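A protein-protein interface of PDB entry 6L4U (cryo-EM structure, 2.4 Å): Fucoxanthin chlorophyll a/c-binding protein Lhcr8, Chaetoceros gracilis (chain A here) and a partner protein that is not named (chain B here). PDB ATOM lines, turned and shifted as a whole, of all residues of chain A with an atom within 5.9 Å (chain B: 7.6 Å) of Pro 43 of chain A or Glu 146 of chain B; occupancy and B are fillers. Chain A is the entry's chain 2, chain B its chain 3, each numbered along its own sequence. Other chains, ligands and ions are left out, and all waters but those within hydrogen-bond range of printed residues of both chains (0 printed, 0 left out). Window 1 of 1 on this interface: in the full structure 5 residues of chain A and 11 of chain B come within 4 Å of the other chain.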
ATOM      1  N   LYS A  34      15.628  -8.186  -7.348  1.00  0.00           N
ATOM      2  CA  LYS A  34      16.239  -7.258  -6.405  1.00  0.00           C
ATOM      3  C   LYS A  34      16.093  -5.838  -6.937  1.00  0.00           C
ATOM      4  O   LYS A  34      15.953  -4.888  -6.170  1.00  0.00           O
ATOM      5  CB  LYS A  34      17.711  -7.617  -6.172  1.00  0.00           C
ATOM      6  CG  LYS A  34      18.419  -6.841  -5.059  1.00  0.00           C
ATOM      7  CD  LYS A  34      19.241  -5.665  -5.580  1.00  0.00           C
ATOM      8  CE  LYS A  34      20.454  -6.125  -6.360  1.00  0.00           C
ATOM      9  NZ  LYS A  34      21.234  -4.962  -6.862  1.00  0.00           N
ATOM     10  N   GLN A  35      16.134  -5.698  -8.254  1.00  0.00           N
ATOM     11  CA  GLN A  35      15.920  -4.416  -8.904  1.00  0.00           C
ATOM     12  C   GLN A  35      14.523  -4.364  -9.504  1.00  0.00           C
ATOM     13  O   GLN A  35      13.965  -5.385  -9.915  1.00  0.00           O
ATOM     14  CB  GLN A  35      16.963  -4.172  -9.993  1.00  0.00           C
ATOM     15  CG  GLN A  35      18.294  -3.679  -9.473  1.00  0.00           C
ATOM     16  CD  GLN A  35      18.363  -2.173  -9.425  1.00  0.00           C
ATOM     17  OE1 GLN A  35      17.955  -1.495 -10.364  1.00  0.00           O
ATOM     18  NE2 GLN A  35      18.875  -1.637  -8.326  1.00  0.00           N
ATOM     19  N   SER A  36      13.961  -3.162  -9.542  1.00  0.00           N
ATOM     20  CA  SER A  36      12.637  -2.968 -10.113  1.00  0.00           C
ATOM     21  C   SER A  36      12.674  -3.143 -11.624  1.00  0.00           C
ATOM     22  O   SER A  36      13.644  -2.765 -12.285  1.00  0.00           O
ATOM     23  CB  SER A  36      12.114  -1.580  -9.759  1.00  0.00           C
ATOM     24  OG  SER A  36      10.833  -1.361 -10.315  1.00  0.00           O
ATOM     25  N   LEU A  39      11.512   0.391 -13.302  1.00  0.00           N
ATOM     26  CA  LEU A  39      12.513   1.416 -13.024  1.00  0.00           C
ATOM     27  C   LEU A  39      13.804   0.702 -12.658  1.00  0.00           C
ATOM     28  O   LEU A  39      14.066   0.446 -11.476  1.00  0.00           O
ATOM     29  CB  LEU A  39      12.052   2.329 -11.895  1.00  0.00           C
ATOM     30  CG  LEU A  39      10.908   3.277 -12.222  1.00  0.00           C
ATOM     31  CD1 LEU A  39      10.308   3.758 -10.959  1.00  0.00           C
ATOM     32  CD2 LEU A  39      11.459   4.458 -12.960  1.00  0.00           C
ATOM     33  N   PHE A  41      16.765   1.234 -11.906  1.00  0.00           N
ATOM     34  CA  PHE A  41      17.795   1.862 -11.094  1.00  0.00           C
ATOM     35  C   PHE A  41      17.392   1.995  -9.639  1.00  0.00           C
ATOM     36  O   PHE A  41      18.259   2.265  -8.801  1.00  0.00           O
ATOM     37  CB  PHE A  41      18.170   3.252 -11.644  1.00  0.00           C
ATOM     38  CG  PHE A  41      16.993   4.146 -11.928  1.00  0.00           C
ATOM     39  CD1 PHE A  41      16.366   4.126 -13.164  1.00  0.00           C
ATOM     40  CD2 PHE A  41      16.539   5.035 -10.969  1.00  0.00           C
ATOM     41  CE1 PHE A  41      15.299   4.944 -13.427  1.00  0.00           C
ATOM     42  CE2 PHE A  41      15.469   5.863 -11.230  1.00  0.00           C
ATOM     43  CZ  PHE A  41      14.851   5.814 -12.464  1.00  0.00           C
ATOM     44  N   LEU A  42      16.150   1.820  -9.321  1.00  0.00           N
ATOM     45  CA  LEU A  42      15.483   1.686  -8.042  1.00  0.00           C
ATOM     46  C   LEU A  42      15.394   0.217  -7.649  1.00  0.00           C
ATOM     47  O   LEU A  42      15.255  -0.653  -8.511  1.00  0.00           O
ATOM     48  CB  LEU A  42      14.082   2.285  -8.103  1.00  0.00           C
ATOM     49  CG  LEU A  42      13.981   3.782  -8.382  1.00  0.00           C
ATOM     50  CD1 LEU A  42      12.589   4.281  -8.082  1.00  0.00           C
ATOM     51  CD2 LEU A  42      14.990   4.539  -7.565  1.00  0.00           C
ATOM     52  N   PRO A  43      15.489  -0.092  -6.359  1.00  0.00           N
ATOM     53  CA  PRO A  43      15.348  -1.483  -5.921  1.00  0.00           C
ATOM     54  C   PRO A  43      13.905  -1.955  -6.015  1.00  0.00           C
ATOM     55  O   PRO A  43      12.969  -1.182  -6.219  1.00  0.00           O
ATOM     56  CB  PRO A  43      15.832  -1.450  -4.471  1.00  0.00           C
ATOM     57  CG  PRO A  43      15.660  -0.041  -4.047  1.00  0.00           C
ATOM     58  CD  PRO A  43      15.903   0.793  -5.258  1.00  0.00           C
ATOM     59  N   TYR A  44      13.740  -3.256  -5.857  1.00  0.00           N
ATOM     60  CA  TYR A  44      12.414  -3.856  -5.916  1.00  0.00           C
ATOM     61  C   TYR A  44      11.671  -3.594  -4.608  1.00  0.00           C
ATOM     62  O   TYR A  44      12.275  -3.684  -3.534  1.00  0.00           O
ATOM     63  CB  TYR A  44      12.549  -5.350  -6.186  1.00  0.00           C
ATOM     64  CG  TYR A  44      11.244  -6.079  -6.342  1.00  0.00           C
ATOM     65  CD1 TYR A  44      10.473  -5.925  -7.485  1.00  0.00           C
ATOM     66  CD2 TYR A  44      10.790  -6.935  -5.352  1.00  0.00           C
ATOM     67  CE1 TYR A  44       9.277  -6.592  -7.629  1.00  0.00           C
ATOM     68  CE2 TYR A  44       9.594  -7.607  -5.485  1.00  0.00           C
ATOM     69  CZ  TYR A  44       8.844  -7.432  -6.625  1.00  0.00           C
ATOM     70  OH  TYR A  44       7.653  -8.105  -6.762  1.00  0.00           O
ATOM     71  N   PRO A  45      10.381  -3.239  -4.651  1.00  0.00           N
ATOM     72  CA  PRO A  45       9.683  -2.822  -3.420  1.00  0.00           C
ATOM     73  C   PRO A  45       9.351  -3.948  -2.444  1.00  0.00           C
ATOM     74  O   PRO A  45       8.886  -3.640  -1.337  1.00  0.00           O
ATOM     75  CB  PRO A  45       8.404  -2.166  -3.953  1.00  0.00           C
ATOM     76  CG  PRO A  45       8.745  -1.765  -5.344  1.00  0.00           C
ATOM     77  CD  PRO A  45       9.617  -2.862  -5.849  1.00  0.00           C
ATOM     78  N   GLY A  56       6.796  -4.304 -10.315  1.00  0.00           N
ATOM     79  CA  GLY A  56       7.807  -3.756  -9.440  1.00  0.00           C
ATOM     80  C   GLY A  56       7.852  -2.254  -9.484  1.00  0.00           C
ATOM     81  O   GLY A  56       8.880  -1.664  -9.150  1.00  0.00           O
ATOM     82  N   ARG A  61       6.573   3.727  -2.742  1.00  0.00           N
ATOM     83  CA  ARG A  61       6.537   2.599  -1.815  1.00  0.00           C
ATOM     84  C   ARG A  61       5.327   2.658  -0.891  1.00  0.00           C
ATOM     85  O   ARG A  61       5.429   2.451   0.314  1.00  0.00           O
ATOM     86  CB  ARG A  61       7.842   2.475  -1.034  1.00  0.00           C
ATOM     87  CG  ARG A  61       8.821   1.600  -1.766  1.00  0.00           C
ATOM     88  CD  ARG A  61      10.248   1.952  -1.469  1.00  0.00           C
ATOM     89  NE  ARG A  61      11.146   1.200  -2.334  1.00  0.00           N
ATOM     90  CZ  ARG A  61      11.559  -0.036  -2.088  1.00  0.00           C
ATOM     91  NH1 ARG A  61      12.374  -0.642  -2.937  1.00  0.00           N
ATOM     92  NH2 ARG A  61      11.164  -0.665  -0.991  1.00  0.00           N
ATOM     93  N   PRO B 137      12.402   9.092  -4.721  1.00  0.00           N
ATOM     94  CA  PRO B 137      12.770   7.710  -4.378  1.00  0.00           C
ATOM     95  C   PRO B 137      14.175   7.322  -4.798  1.00  0.00           C
ATOM     96  O   PRO B 137      14.706   6.343  -4.265  1.00  0.00           O
ATOM     97  CB  PRO B 137      11.722   6.873  -5.116  1.00  0.00           C
ATOM     98  CG  PRO B 137      10.574   7.743  -5.185  1.00  0.00           C
ATOM     99  CD  PRO B 137      11.150   9.075  -5.506  1.00  0.00           C
ATOM    100  N   ALA B 138      14.791   8.038  -5.738  1.00  0.00           N
ATOM    101  CA  ALA B 138      16.157   7.710  -6.119  1.00  0.00           C
ATOM    102  C   ALA B 138      17.159   8.177  -5.075  1.00  0.00           C
ATOM    103  O   ALA B 138      18.116   7.461  -4.772  1.00  0.00           O
ATOM    104  CB  ALA B 138      16.485   8.308  -7.486  1.00  0.00           C
ATOM    105  N   GLN B 140      16.605   8.538  -1.883  1.00  0.00           N
ATOM    106  CA  GLN B 140      16.524   7.752  -0.662  1.00  0.00           C
ATOM    107  C   GLN B 140      17.071   6.348  -0.844  1.00  0.00           C
ATOM    108  O   GLN B 140      17.523   5.746   0.133  1.00  0.00           O
ATOM    109  CB  GLN B 140      15.088   7.678  -0.125  1.00  0.00           C
ATOM    110  CG  GLN B 140      14.110   6.856  -0.929  1.00  0.00           C
ATOM    111  CD  GLN B 140      12.761   6.746  -0.248  1.00  0.00           C
ATOM    112  OE1 GLN B 140      12.570   7.250   0.857  1.00  0.00           O
ATOM    113  NE2 GLN B 140      11.819   6.071  -0.899  1.00  0.00           N
ATOM    114  N   ALA B 141      17.059   5.822  -2.069  1.00  0.00           N
ATOM    115  CA  ALA B 141      17.746   4.569  -2.344  1.00  0.00           C
ATOM    116  C   ALA B 141      19.250   4.770  -2.409  1.00  0.00           C
ATOM    117  O   ALA B 141      20.010   3.831  -2.158  1.00  0.00           O
ATOM    118  CB  ALA B 141      17.236   3.958  -3.647  1.00  0.00           C
ATOM    119  N   MET B 142      19.690   5.984  -2.734  1.00  0.00           N
ATOM    120  CA  MET B 142      21.112   6.296  -2.698  1.00  0.00           C
ATOM    121  C   MET B 142      21.611   6.384  -1.264  1.00  0.00           C
ATOM    122  O   MET B 142      22.722   5.937  -0.958  1.00  0.00           O
ATOM    123  CB  MET B 142      21.372   7.602  -3.447  1.00  0.00           C
ATOM    124  CG  MET B 142      22.827   8.020  -3.507  1.00  0.00           C
ATOM    125  SD  MET B 142      23.256   9.255  -2.272  1.00  0.00           S
ATOM    126  CE  MET B 142      21.975  10.469  -2.545  1.00  0.00           C
ATOM    127  N   GLY B 143      20.804   6.963  -0.373  1.00  0.00           N
ATOM    128  CA  GLY B 143      21.175   7.023   1.027  1.00  0.00           C
ATOM    129  C   GLY B 143      21.142   5.674   1.710  1.00  0.00           C
ATOM    130  O   GLY B 143      21.899   5.435   2.652  1.00  0.00           O
ATOM    131  N   LYS B 144      20.274   4.777   1.248  1.00  0.00           N
ATOM    132  CA  LYS B 144      20.273   3.416   1.763  1.00  0.00           C
ATOM    133  C   LYS B 144      21.394   2.576   1.171  1.00  0.00           C
ATOM    134  O   LYS B 144      21.742   1.540   1.745  1.00  0.00           O
ATOM    135  CB  LYS B 144      18.915   2.758   1.505  1.00  0.00           C
ATOM    136  CG  LYS B 144      17.789   3.329   2.361  1.00  0.00           C
ATOM    137  CD  LYS B 144      16.477   2.581   2.159  1.00  0.00           C
ATOM    138  CE  LYS B 144      15.804   2.975   0.849  1.00  0.00           C
ATOM    139  NZ  LYS B 144      14.477   2.326   0.668  1.00  0.00           N
ATOM    140  N   GLY B 145      21.966   3.000   0.049  1.00  0.00           N
ATOM    141  CA  GLY B 145      23.149   2.372  -0.495  1.00  0.00           C
ATOM    142  C   GLY B 145      22.937   1.395  -1.627  1.00  0.00           C
ATOM    143  O   GLY B 145      23.867   0.645  -1.947  1.00  0.00           O
ATOM    144  N   GLU B 146      21.758   1.369  -2.247  1.00  0.00           N
ATOM    145  CA  GLU B 146      21.515   0.400  -3.307  1.00  0.00           C
ATOM    146  C   GLU B 146      21.503   1.000  -4.707  1.00  0.00           C
ATOM    147  O   GLU B 146      21.314   0.255  -5.673  1.00  0.00           O
ATOM    148  CB  GLU B 146      20.203  -0.348  -3.068  1.00  0.00           C
ATOM    149  CG  GLU B 146      19.036   0.518  -2.683  1.00  0.00           C
ATOM    150  CD  GLU B 146      18.738   0.439  -1.206  1.00  0.00           C
ATOM    151  OE1 GLU B 146      19.645   0.058  -0.439  1.00  0.00           O
ATOM    152  OE2 GLU B 146      17.592   0.735  -0.811  1.00  0.00           O
ATOM    153  N   ARG B 147      21.690   2.308  -4.855  1.00  0.00           N
ATOM    154  CA  ARG B 147      21.975   2.857  -6.172  1.00  0.00           C
ATOM    155  C   ARG B 147      23.078   3.894  -6.057  1.00  0.00           C
ATOM    156  O   ARG B 147      23.245   4.529  -5.012  1.00  0.00           O
ATOM    157  CB  ARG B 147      20.740   3.472  -6.842  1.00  0.00           C
ATOM    158  CG  ARG B 147      20.184   4.705  -6.187  1.00  0.00           C
ATOM    159  CD  ARG B 147      19.118   5.337  -7.064  1.00  0.00           C
ATOM    160  NE  ARG B 147      19.664   6.100  -8.181  1.00  0.00           N
ATOM    161  CZ  ARG B 147      20.020   7.379  -8.106  1.00  0.00           C
ATOM    162  NH1 ARG B 147      19.899   8.037  -6.965  1.00  0.00           N
ATOM    163  NH2 ARG B 147      20.503   8.002  -9.167  1.00  0.00           N
ATOM    164  N   GLU B 148      23.845   4.034  -7.126  1.00  0.00           N
ATOM    165  CA  GLU B 148      24.894   5.032  -7.234  1.00  0.00           C
ATOM    166  C   GLU B 148      24.283   6.401  -7.503  1.00  0.00           C
ATOM    167  O   GLU B 148      23.245   6.494  -8.161  1.00  0.00           O
ATOM    168  CB  GLU B 148      25.860   4.673  -8.353  1.00  0.00           C
ATOM    169  CG  GLU B 148      26.608   3.381  -8.105  1.00  0.00           C
ATOM    170  CD  GLU B 148      27.568   3.480  -6.939  1.00  0.00           C
ATOM    171  OE1 GLU B 148      28.145   4.568  -6.726  1.00  0.00           O
ATOM    172  OE2 GLU B 148      27.745   2.467  -6.231  1.00  0.00           O
ATOM    173  N   ASP B 151      22.864   7.847 -11.212  1.00  0.00           N
ATOM    174  CA  ASP B 151      22.395   6.759 -12.061  1.00  0.00           C
ATOM    175  C   ASP B 151      20.877   6.811 -12.170  1.00  0.00           C
ATOM    176  O   ASP B 151      20.167   6.547 -11.195  1.00  0.00           O
ATOM    177  CB  ASP B 151      22.852   5.417 -11.501  1.00  0.00           C
ATOM    178  CG  ASP B 151      22.329   4.245 -12.302  1.00  0.00           C
ATOM    179  OD1 ASP B 151      22.252   4.357 -13.543  1.00  0.00           O
ATOM    180  OD2 ASP B 151      21.994   3.210 -11.693  1.00  0.00           O
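Printed residues of chain B within 4 Å of Phe 41 of chain A: Arg 147 (3.4 Å) and Asp 151 (3.8 Å).
Of the printed residues of chain B, Leu 42 of chain A touches Pro 137 and Ala 138.
Of chain B, only Ala 141 and Glu 146 come within 4 Å of Pro 43 of chain A.
Of the printed residues of chain A, Ala 138 of chain B touches Leu 42 (3.7 Å).
Gln 140 of chain B touches none of the printed residues of chain A.
Met 142 of chain B touches none of the printed residues of chain A.
Of the printed residues of chain A, Arg 147 of chain B touches Phe 41 (3.4 Å).
Of the printed residues of chain A, Asp 151 of chain B touches Phe 41.
The nearest residue of chain A that does not touch Glu 146 of chain B is Gln 35 of chain A (4.1 Å).
The nearest printed residue of chain A that does not touch Ala 138 of chain B is Phe 41 of chain A (4.6 Å).
Of the 12 printed residues of chain B, 6 touch a printed residue of chain A.
Printed residues of chain B that touch a printed residue of chain A: Pro 137, Ala 138, Ala 141, Glu 146, Arg 147 and Asp 151.
Of the 11 printed residues of chain A, 3 touch a printed residue of chain B.
Printed residues of chain A that touch a printed residue of chain B: Phe 41, Leu 42 and Pro 43.
Among the printed residues, 6 pairs touch across the chains.
Among the printed residues, no Asp or Glu carboxylate lies within 4 Å of a Lys or Arg side-chain nitrogen of the other chain.
The backbone carbonyl oxygen (O) of Asp 151 of chain B sits at hydrogen-bond distance from the guanidinium group (NH2) of Arg 147 of chain B.
The backbone carbonyl oxygen of Pro 43 of chain A lies within hydrogen-bond range of the guanidinium group of Arg 61 of chain A (3.4 Å).
The backbone NH (N) of Phe 41 of chain A lies within hydrogen-bond range of the side-chain amide oxygen (OE1) of Gln 35 of chain A, at 3.4 Å.
The side-chain carboxylate (OE2) of Glu 146 of chain B lies within salt-bridge range of the side-chain amino group (NZ) of Lys 144 of chain B (3.8 Å).
N of Ser 36 of chain A lies within hydrogen-bond range of O of Leu 42 of chain A (3.0 Å).
The backbone carbonyl oxygen (O) of Ala 138 of chain B is in hydrogen-bond range of the guanidinium group (NH1) of Arg 147 of chain B, 2.9 Å away.
Among the printed residues, merely in contact across the chains: Phe 41 of chain A with Arg 147 of chain B (3.4 Å), Phe 41 of chain A with Asp 151 of chain B (3.8 Å), Leu 42 of chain A with Pro 137 of chain B (3.8 Å), Leu 42 of chain A with Ala 138 of chain B (3.7 Å), Pro 43 of chain A with Ala 141 of chain B (3.8 Å) and Pro 43 of chain A with Glu 146 of chain B (3.7 Å).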
